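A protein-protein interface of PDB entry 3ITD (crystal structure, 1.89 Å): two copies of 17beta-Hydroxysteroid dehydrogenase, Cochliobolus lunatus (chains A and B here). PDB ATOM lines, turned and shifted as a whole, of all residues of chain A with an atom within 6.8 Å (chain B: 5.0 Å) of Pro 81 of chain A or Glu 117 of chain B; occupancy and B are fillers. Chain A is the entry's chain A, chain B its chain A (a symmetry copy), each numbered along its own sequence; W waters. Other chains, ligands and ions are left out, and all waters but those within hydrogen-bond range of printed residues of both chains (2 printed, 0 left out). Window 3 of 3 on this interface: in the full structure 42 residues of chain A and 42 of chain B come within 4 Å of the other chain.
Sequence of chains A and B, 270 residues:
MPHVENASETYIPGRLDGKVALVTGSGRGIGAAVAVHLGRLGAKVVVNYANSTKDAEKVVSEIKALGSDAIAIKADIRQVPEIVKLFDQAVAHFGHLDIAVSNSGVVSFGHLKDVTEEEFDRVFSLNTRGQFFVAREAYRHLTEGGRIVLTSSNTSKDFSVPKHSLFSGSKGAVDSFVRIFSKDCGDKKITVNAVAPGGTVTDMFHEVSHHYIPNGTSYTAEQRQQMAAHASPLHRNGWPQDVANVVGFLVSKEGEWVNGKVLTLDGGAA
Of the 13 printed residues of chain A, 5 touch a printed residue of chain B. Printed residues of chain A that touch a printed residue of chain B: Val 80, Pro 81, Arg 129, Phe 133 and Arg 136. Hydrophobic or aromatic side chains of chain A within 4 Å of the printed part of chain B: Val 80, Pro 81 and Phe 133. Of the 7 printed residues of chain B, 5 touch a printed residue of chain A. Printed residues of chain B that touch a printed residue of chain A: Val 115, Thr 116, Glu 117, Phe 120 and Asp 121. Among the printed residues, 10 pairs touch across the chains. Among the printed residues, Asp or Glu carboxylates within 4 Å of a Lys or Arg side-chain nitrogen of the other chain: Arg 129 of chain A with Glu 117 of chain B (2.9 Å) and Arg 129 of chain A with Asp 121 of chain B (2.8 Å).
Among the printed residues, pairs that only touch across the chains: Phe 133 of chain A with Val 115 of chain B, Arg 129 of chain A with Phe 120 of chain B, Phe 133 of chain A with Thr 116 of chain B, Phe 133 of chain A with Phe 120 of chain B, Val 80 of chain A with Glu 117 of chain B, Phe 133 of chain A with Glu 117 of chain B and Pro 81 of chain A with Glu 117 of chain B.
The backbone NH of Glu 118 of chain B sits close to the side-chain hydroxyl of Thr 116 of chain B. OG1 of Thr 116 of chain B is in hydrogen-bond range of N of Glu 119 of chain B, at 3.0 Å.
Asp 76 of chain A touches none of the printed residues of chain B. Gln 79 of chain A touches none of the printed residues of chain B. Pro 81 of chain A touches just one residue of chain B: Glu 117 (3.8 Å). Of the printed residues of chain B, Arg 129 of chain A touches Glu 117 (2.9 Å), Phe 120 (3.5 Å) and Asp 121 (2.8 Å). Of the printed residues of chain B, Arg 136 of chain A touches Val 115. Glu 117 of chain B touches just these residues of chain A: Val 80 (3.7 Å), Pro 81 (3.8 Å), Arg 129 (2.9 Å) and Phe 133 (3.7 Å). The nearest printed residue of chain A that does not touch Phe 120 of chain B is Val 80 of chain A (7.6 Å).
Water W2 lies within hydrogen-bond range of OE1 of Glu 117 of chain B (2.7 Å), N of Val 80 of chain A (2.9 Å), NH1 of Arg 129 of chain A (3.2 Å) and O of Arg 78 of chain A (3.4 Å). Water W1 bridges the backbone NH of Glu 117 of chain B (3.1 Å) and the guanidinium group of Arg 136 of chain A (3.2 Å).
No position is printed for both chains. Of the 10 pairs that touch across the chains among the printed residues, none has its exchanged pair printed and touching as well.
The guanidinium group of Arg 129 of chain A is in salt-bridge range of the side-chain carboxylate of Glu 117 of chain B, 2.9 Å away. OD1 of Asp 121 of chain B lies within salt-bridge range of NE of Arg 129 of chain A (2.8 Å). The guanidinium group (NH1) of Arg 136 of chain A sits at hydrogen-bond distance from the backbone carbonyl oxygen (O) of Val 115 of chain B (2.8 Å).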
ATOM      1  N   ASP A  76     -10.569  -7.379 -36.357  1.00  0.00           N
ATOM      2  CA  ASP A  76      -9.584  -6.600 -35.595  1.00  0.00           C
ATOM      3  C   ASP A  76      -9.934  -6.678 -34.090  1.00  0.00           C
ATOM      4  O   ASP A  76     -10.834  -5.982 -33.605  1.00  0.00           O
ATOM      5  CB  ASP A  76      -9.566  -5.149 -36.107  1.00  0.00           C
ATOM      6  CG  ASP A  76      -8.532  -4.278 -35.399  1.00  0.00           C
ATOM      7  OD1 ASP A  76      -7.858  -4.761 -34.473  1.00  0.00           O
ATOM      8  OD2 ASP A  76      -8.414  -3.090 -35.762  1.00  0.00           O
ATOM      9  N   ARG A  78      -8.443  -5.578 -31.558  1.00  0.00           N
ATOM     10  CA  ARG A  78      -8.328  -4.296 -30.879  1.00  0.00           C
ATOM     11  C   ARG A  78      -9.658  -3.533 -30.785  1.00  0.00           C
ATOM     12  O   ARG A  78      -9.823  -2.665 -29.914  1.00  0.00           O
ATOM     13  CB  ARG A  78      -7.261  -3.397 -31.535  1.00  0.00           C
ATOM     14  CG  ARG A  78      -5.812  -3.908 -31.303  1.00  0.00           C
ATOM     15  CD  ARG A  78      -4.753  -2.852 -31.751  1.00  0.00           C
ATOM     16  NE  ARG A  78      -3.408  -3.291 -31.335  1.00  0.00           N
ATOM     17  CZ  ARG A  78      -2.605  -4.025 -32.095  1.00  0.00           C
ATOM     18  NH1 ARG A  78      -2.989  -4.386 -33.322  1.00  0.00           N
ATOM     19  NH2 ARG A  78      -1.413  -4.378 -31.641  1.00  0.00           N
ATOM     20  N   GLN A  79     -10.591  -3.825 -31.696  1.00  0.00           N
ATOM     21  CA  GLN A  79     -11.876  -3.147 -31.716  1.00  0.00           C
ATOM     22  C   GLN A  79     -12.948  -4.051 -31.133  1.00  0.00           C
ATOM     23  O   GLN A  79     -13.375  -5.035 -31.764  1.00  0.00           O
ATOM     24  CB  GLN A  79     -12.252  -2.737 -33.144  1.00  0.00           C
ATOM     25  CG  GLN A  79     -11.251  -1.764 -33.772  1.00  0.00           C
ATOM     26  CD  GLN A  79     -11.708  -1.262 -35.122  1.00  0.00           C
ATOM     27  OE1 GLN A  79     -12.858  -0.866 -35.293  1.00  0.00           O
ATOM     28  NE2 GLN A  79     -10.803  -1.273 -36.095  1.00  0.00           N
ATOM     29  N   VAL A  80     -13.388  -3.711 -29.925  1.00  0.00           N
ATOM     30  CA  VAL A  80     -14.397  -4.528 -29.233  1.00  0.00           C
ATOM     31  C   VAL A  80     -15.684  -4.760 -30.066  1.00  0.00           C
ATOM     32  O   VAL A  80     -16.196  -5.885 -30.078  1.00  0.00           O
ATOM     33  CB  VAL A  80     -14.658  -3.993 -27.794  1.00  0.00           C
ATOM     34  CG1 VAL A  80     -15.813  -4.756 -27.098  1.00  0.00           C
ATOM     35  CG2 VAL A  80     -13.342  -4.088 -26.991  1.00  0.00           C
ATOM     36  N   PRO A  81     -16.191  -3.725 -30.791  1.00  0.00           N
ATOM     37  CA  PRO A  81     -17.345  -4.031 -31.650  1.00  0.00           C
ATOM     38  C   PRO A  81     -17.092  -5.135 -32.679  1.00  0.00           C
ATOM     39  O   PRO A  81     -18.052  -5.823 -33.095  1.00  0.00           O
ATOM     40  CB  PRO A  81     -17.615  -2.706 -32.396  1.00  0.00           C
ATOM     41  CG  PRO A  81     -17.071  -1.645 -31.475  1.00  0.00           C
ATOM     42  CD  PRO A  81     -15.917  -2.271 -30.727  1.00  0.00           C
ATOM     43  N   GLU A  82     -15.846  -5.283 -33.139  1.00  0.00           N
ATOM     44  CA  GLU A  82     -15.564  -6.367 -34.098  1.00  0.00           C
ATOM     45  C   GLU A  82     -15.527  -7.721 -33.415  1.00  0.00           C
ATOM     46  O   GLU A  82     -15.866  -8.729 -34.043  1.00  0.00           O
ATOM     47  CB  GLU A  82     -14.280  -6.110 -34.880  1.00  0.00           C
ATOM     48  CG  GLU A  82     -14.328  -4.787 -35.651  1.00  0.00           C
ATOM     49  CD  GLU A  82     -13.256  -4.699 -36.761  1.00  0.00           C
ATOM     50  OE1 GLU A  82     -12.699  -5.759 -37.173  1.00  0.00           O
ATOM     51  OE2 GLU A  82     -12.988  -3.565 -37.234  1.00  0.00           O
ATOM     52  N   ILE A  83     -15.127  -7.750 -32.136  1.00  0.00           N
ATOM     53  CA  ILE A  83     -15.189  -8.996 -31.347  1.00  0.00           C
ATOM     54  C   ILE A  83     -16.658  -9.447 -31.221  1.00  0.00           C
ATOM     55  O   ILE A  83     -16.955 -10.603 -31.445  1.00  0.00           O
ATOM     56  CB  ILE A  83     -14.547  -8.867 -29.946  1.00  0.00           C
ATOM     57  CG1 ILE A  83     -13.089  -8.364 -30.076  1.00  0.00           C
ATOM     58  CG2 ILE A  83     -14.562 -10.238 -29.207  1.00  0.00           C
ATOM     59  CD1 ILE A  83     -12.427  -7.933 -28.731  1.00  0.00           C
ATOM     60  N   VAL A  84     -17.547  -8.535 -30.852  1.00  0.00           N
ATOM     61  CA  VAL A  84     -18.990  -8.824 -30.781  1.00  0.00           C
ATOM     62  C   VAL A  84     -19.494  -9.451 -32.111  1.00  0.00           C
ATOM     63  O   VAL A  84     -20.130 -10.520 -32.120  1.00  0.00           O
ATOM     64  CB  VAL A  84     -19.813  -7.531 -30.401  1.00  0.00           C
ATOM     65  CG1 VAL A  84     -21.323  -7.788 -30.477  1.00  0.00           C
ATOM     66  CG2 VAL A  84     -19.408  -6.974 -28.984  1.00  0.00           C
ATOM     67  N   LYS A  85     -19.206  -8.786 -33.232  1.00  0.00           N
ATOM     68  CA  LYS A  85     -19.642  -9.285 -34.542  1.00  0.00           C
ATOM     69  C   LYS A  85     -19.057 -10.651 -34.877  1.00  0.00           C
ATOM     70  O   LYS A  85     -19.765 -11.509 -35.401  1.00  0.00           O
ATOM     71  CB  LYS A  85     -19.331  -8.303 -35.677  1.00  0.00           C
ATOM     72  CG  LYS A  85     -20.197  -7.064 -35.676  1.00  0.00           C
ATOM     73  CD  LYS A  85     -20.093  -6.316 -37.013  1.00  0.00           C
ATOM     74  CE  LYS A  85     -20.653  -4.905 -36.898  1.00  0.00           C
ATOM     75  NZ  LYS A  85     -20.547  -4.149 -38.177  1.00  0.00           N
ATOM     76  N   LEU A  86     -17.777 -10.855 -34.566  1.00  0.00           N
ATOM     77  CA  LEU A  86     -17.141 -12.149 -34.798  1.00  0.00           C
ATOM     78  C   LEU A  86     -17.928 -13.285 -34.116  1.00  0.00           C
ATOM     79  O   LEU A  86     -18.270 -14.288 -34.751  1.00  0.00           O
ATOM     80  CB  LEU A  86     -15.689 -12.122 -34.290  1.00  0.00           C
ATOM     81  CG  LEU A  86     -14.940 -13.467 -34.093  1.00  0.00           C
ATOM     82  CD1 LEU A  86     -14.806 -14.234 -35.417  1.00  0.00           C
ATOM     83  CD2 LEU A  86     -13.562 -13.252 -33.475  1.00  0.00           C
ATOM     84  N   ARG A 129      -6.218  -5.997 -23.235  1.00  0.00           N
ATOM     85  CA  ARG A 129      -7.584  -5.552 -23.511  1.00  0.00           C
ATOM     86  C   ARG A 129      -8.306  -6.458 -24.525  1.00  0.00           C
ATOM     87  O   ARG A 129      -9.420  -6.919 -24.271  1.00  0.00           O
ATOM     88  CB  ARG A 129      -7.566  -4.098 -24.014  1.00  0.00           C
ATOM     89  CG  ARG A 129      -8.927  -3.368 -24.041  1.00  0.00           C
ATOM     90  CD  ARG A 129      -8.620  -1.903 -24.443  1.00  0.00           C
ATOM     91  NE  ARG A 129      -9.756  -0.961 -24.374  1.00  0.00           N
ATOM     92  CZ  ARG A 129     -10.684  -0.872 -25.325  1.00  0.00           C
ATOM     93  NH1 ARG A 129     -10.635  -1.694 -26.377  1.00  0.00           N
ATOM     94  NH2 ARG A 129     -11.633   0.049 -25.236  1.00  0.00           N
ATOM     95  N   PHE A 133     -11.651  -8.899 -23.777  1.00  0.00           N
ATOM     96  CA  PHE A 133     -12.977  -8.800 -24.388  1.00  0.00           C
ATOM     97  C   PHE A 133     -13.365 -10.007 -25.256  1.00  0.00           C
ATOM     98  O   PHE A 133     -14.562 -10.272 -25.491  1.00  0.00           O
ATOM     99  CB  PHE A 133     -13.165  -7.441 -25.100  1.00  0.00           C
ATOM    100  CG  PHE A 133     -13.353  -6.310 -24.120  1.00  0.00           C
ATOM    101  CD1 PHE A 133     -14.567  -6.184 -23.425  1.00  0.00           C
ATOM    102  CD2 PHE A 133     -12.286  -5.439 -23.803  1.00  0.00           C
ATOM    103  CE1 PHE A 133     -14.758  -5.144 -22.469  1.00  0.00           C
ATOM    104  CE2 PHE A 133     -12.452  -4.396 -22.861  1.00  0.00           C
ATOM    105  CZ  PHE A 133     -13.697  -4.248 -22.188  1.00  0.00           C
ATOM    106  N   ARG A 136     -14.902 -11.987 -22.600  1.00  0.00           N
ATOM    107  CA  ARG A 136     -16.245 -11.486 -22.291  1.00  0.00           C
ATOM    108  C   ARG A 136     -17.258 -11.979 -23.335  1.00  0.00           C
ATOM    109  O   ARG A 136     -18.364 -12.473 -22.995  1.00  0.00           O
ATOM    110  CB  ARG A 136     -16.268  -9.943 -22.224  1.00  0.00           C
ATOM    111  CG  ARG A 136     -17.641  -9.379 -21.783  1.00  0.00           C
ATOM    112  CD  ARG A 136     -17.751  -7.891 -22.033  1.00  0.00           C
ATOM    113  NE  ARG A 136     -18.078  -7.593 -23.430  1.00  0.00           N
ATOM    114  CZ  ARG A 136     -18.261  -6.367 -23.925  1.00  0.00           C
ATOM    115  NH1 ARG A 136     -18.140  -5.306 -23.124  1.00  0.00           N
ATOM    116  NH2 ARG A 136     -18.565  -6.201 -25.230  1.00  0.00           N
ATOM    117  N   VAL B 115     -18.637  -6.006 -17.920  1.00  0.00           N
ATOM    118  CA  VAL B 115     -17.549  -5.027 -17.984  1.00  0.00           C
ATOM    119  C   VAL B 115     -17.557  -4.305 -19.339  1.00  0.00           C
ATOM    120  O   VAL B 115     -17.536  -4.962 -20.398  1.00  0.00           O
ATOM    121  CB  VAL B 115     -16.155  -5.666 -17.715  1.00  0.00           C
ATOM    122  CG1 VAL B 115     -15.023  -4.609 -17.824  1.00  0.00           C
ATOM    123  CG2 VAL B 115     -16.099  -6.318 -16.309  1.00  0.00           C
ATOM    124  N   THR B 116     -17.598  -2.976 -19.302  1.00  0.00           N
ATOM    125  CA  THR B 116     -17.616  -2.158 -20.517  1.00  0.00           C
ATOM    126  C   THR B 116     -16.201  -1.752 -20.951  1.00  0.00           C
ATOM    127  O   THR B 116     -15.255  -1.785 -20.150  1.00  0.00           O
ATOM    128  CB  THR B 116     -18.438  -0.853 -20.323  1.00  0.00           C
ATOM    129  OG1 THR B 116     -17.784  -0.025 -19.338  1.00  0.00           O
ATOM    130  CG2 THR B 116     -19.939  -1.163 -19.916  1.00  0.00           C
ATOM    131  N   GLU B 117     -16.070  -1.363 -22.225  1.00  0.00           N
ATOM    132  CA  GLU B 117     -14.860  -0.726 -22.733  1.00  0.00           C
ATOM    133  C   GLU B 117     -14.438   0.447 -21.857  1.00  0.00           C
ATOM    134  O   GLU B 117     -13.250   0.619 -21.555  1.00  0.00           O
ATOM    135  CB  GLU B 117     -15.157  -0.134 -24.123  1.00  0.00           C
ATOM    136  CG  GLU B 117     -15.165  -1.147 -25.249  1.00  0.00           C
ATOM    137  CD  GLU B 117     -15.044  -0.449 -26.600  1.00  0.00           C
ATOM    138  OE1 GLU B 117     -14.000   0.186 -26.857  1.00  0.00           O
ATOM    139  OE2 GLU B 117     -15.971  -0.542 -27.398  1.00  0.00           O
ATOM    140  N   GLU B 118     -15.415   1.277 -21.490  1.00  0.00           N
ATOM    141  CA  GLU B 118     -15.136   2.485 -20.706  1.00  0.00           C
ATOM    142  C   GLU B 118     -14.561   2.152 -19.324  1.00  0.00           C
ATOM    143  O   GLU B 118     -13.637   2.823 -18.839  1.00  0.00           O
ATOM    144  CB  GLU B 118     -16.393   3.349 -20.562  1.00  0.00           C
ATOM    145  CG  GLU B 118     -16.843   4.025 -21.878  1.00  0.00           C
ATOM    146  CD  GLU B 118     -17.710   3.139 -22.824  1.00  0.00           C
ATOM    147  OE1 GLU B 118     -18.220   3.701 -23.820  1.00  0.00           O
ATOM    148  OE2 GLU B 118     -17.911   1.917 -22.615  1.00  0.00           O
ATOM    149  N   GLU B 119     -15.104   1.118 -18.694  1.00  0.00           N
ATOM    150  CA  GLU B 119     -14.639   0.713 -17.359  1.00  0.00           C
ATOM    151  C   GLU B 119     -13.230   0.106 -17.414  1.00  0.00           C
ATOM    152  O   GLU B 119     -12.374   0.411 -16.560  1.00  0.00           O
ATOM    153  CB  GLU B 119     -15.646  -0.215 -16.657  1.00  0.00           C
ATOM    154  CG  GLU B 119     -15.262  -0.582 -15.190  1.00  0.00           C
ATOM    155  CD  GLU B 119     -15.255   0.615 -14.198  1.00  0.00           C
ATOM    156  OE1 GLU B 119     -14.857   0.392 -13.031  1.00  0.00           O
ATOM    157  OE2 GLU B 119     -15.649   1.764 -14.551  1.00  0.00           O
ATOM    158  N   PHE B 120     -12.988  -0.759 -18.414  1.00  0.00           N
ATOM    159  CA  PHE B 120     -11.683  -1.334 -18.601  1.00  0.00           C
ATOM    160  C   PHE B 120     -10.666  -0.200 -18.728  1.00  0.00           C
ATOM    161  O   PHE B 120      -9.639  -0.209 -18.060  1.00  0.00           O
ATOM    162  CB  PHE B 120     -11.617  -2.253 -19.855  1.00  0.00           C
ATOM    163  CG  PHE B 120     -10.273  -2.905 -20.037  1.00  0.00           C
ATOM    164  CD1 PHE B 120      -9.164  -2.157 -20.473  1.00  0.00           C
ATOM    165  CD2 PHE B 120     -10.108  -4.268 -19.762  1.00  0.00           C
ATOM    166  CE1 PHE B 120      -7.895  -2.753 -20.628  1.00  0.00           C
ATOM    167  CE2 PHE B 120      -8.863  -4.881 -19.906  1.00  0.00           C
ATOM    168  CZ  PHE B 120      -7.744  -4.123 -20.324  1.00  0.00           C
ATOM    169  N   ASP B 121     -10.938   0.770 -19.600  1.00  0.00           N
ATOM    170  CA  ASP B 121     -10.022   1.916 -19.755  1.00  0.00           C
ATOM    171  C   ASP B 121      -9.828   2.809 -18.514  1.00  0.00           C
ATOM    172  O   ASP B 121      -8.696   3.230 -18.233  1.00  0.00           O
ATOM    173  CB  ASP B 121     -10.424   2.752 -20.970  1.00  0.00           C
ATOM    174  CG  ASP B 121     -10.230   1.989 -22.289  1.00  0.00           C
ATOM    175  OD1 ASP B 121      -9.500   0.964 -22.297  1.00  0.00           O
ATOM    176  OD2 ASP B 121     -10.853   2.390 -23.290  1.00  0.00           O
HETATM  177  O   HOH W   1     -18.535  -2.248 -23.897  1.00  0.00           O
HETATM  178  O   HOH W   2     -12.652  -1.181 -28.766  1.00  0.00           O
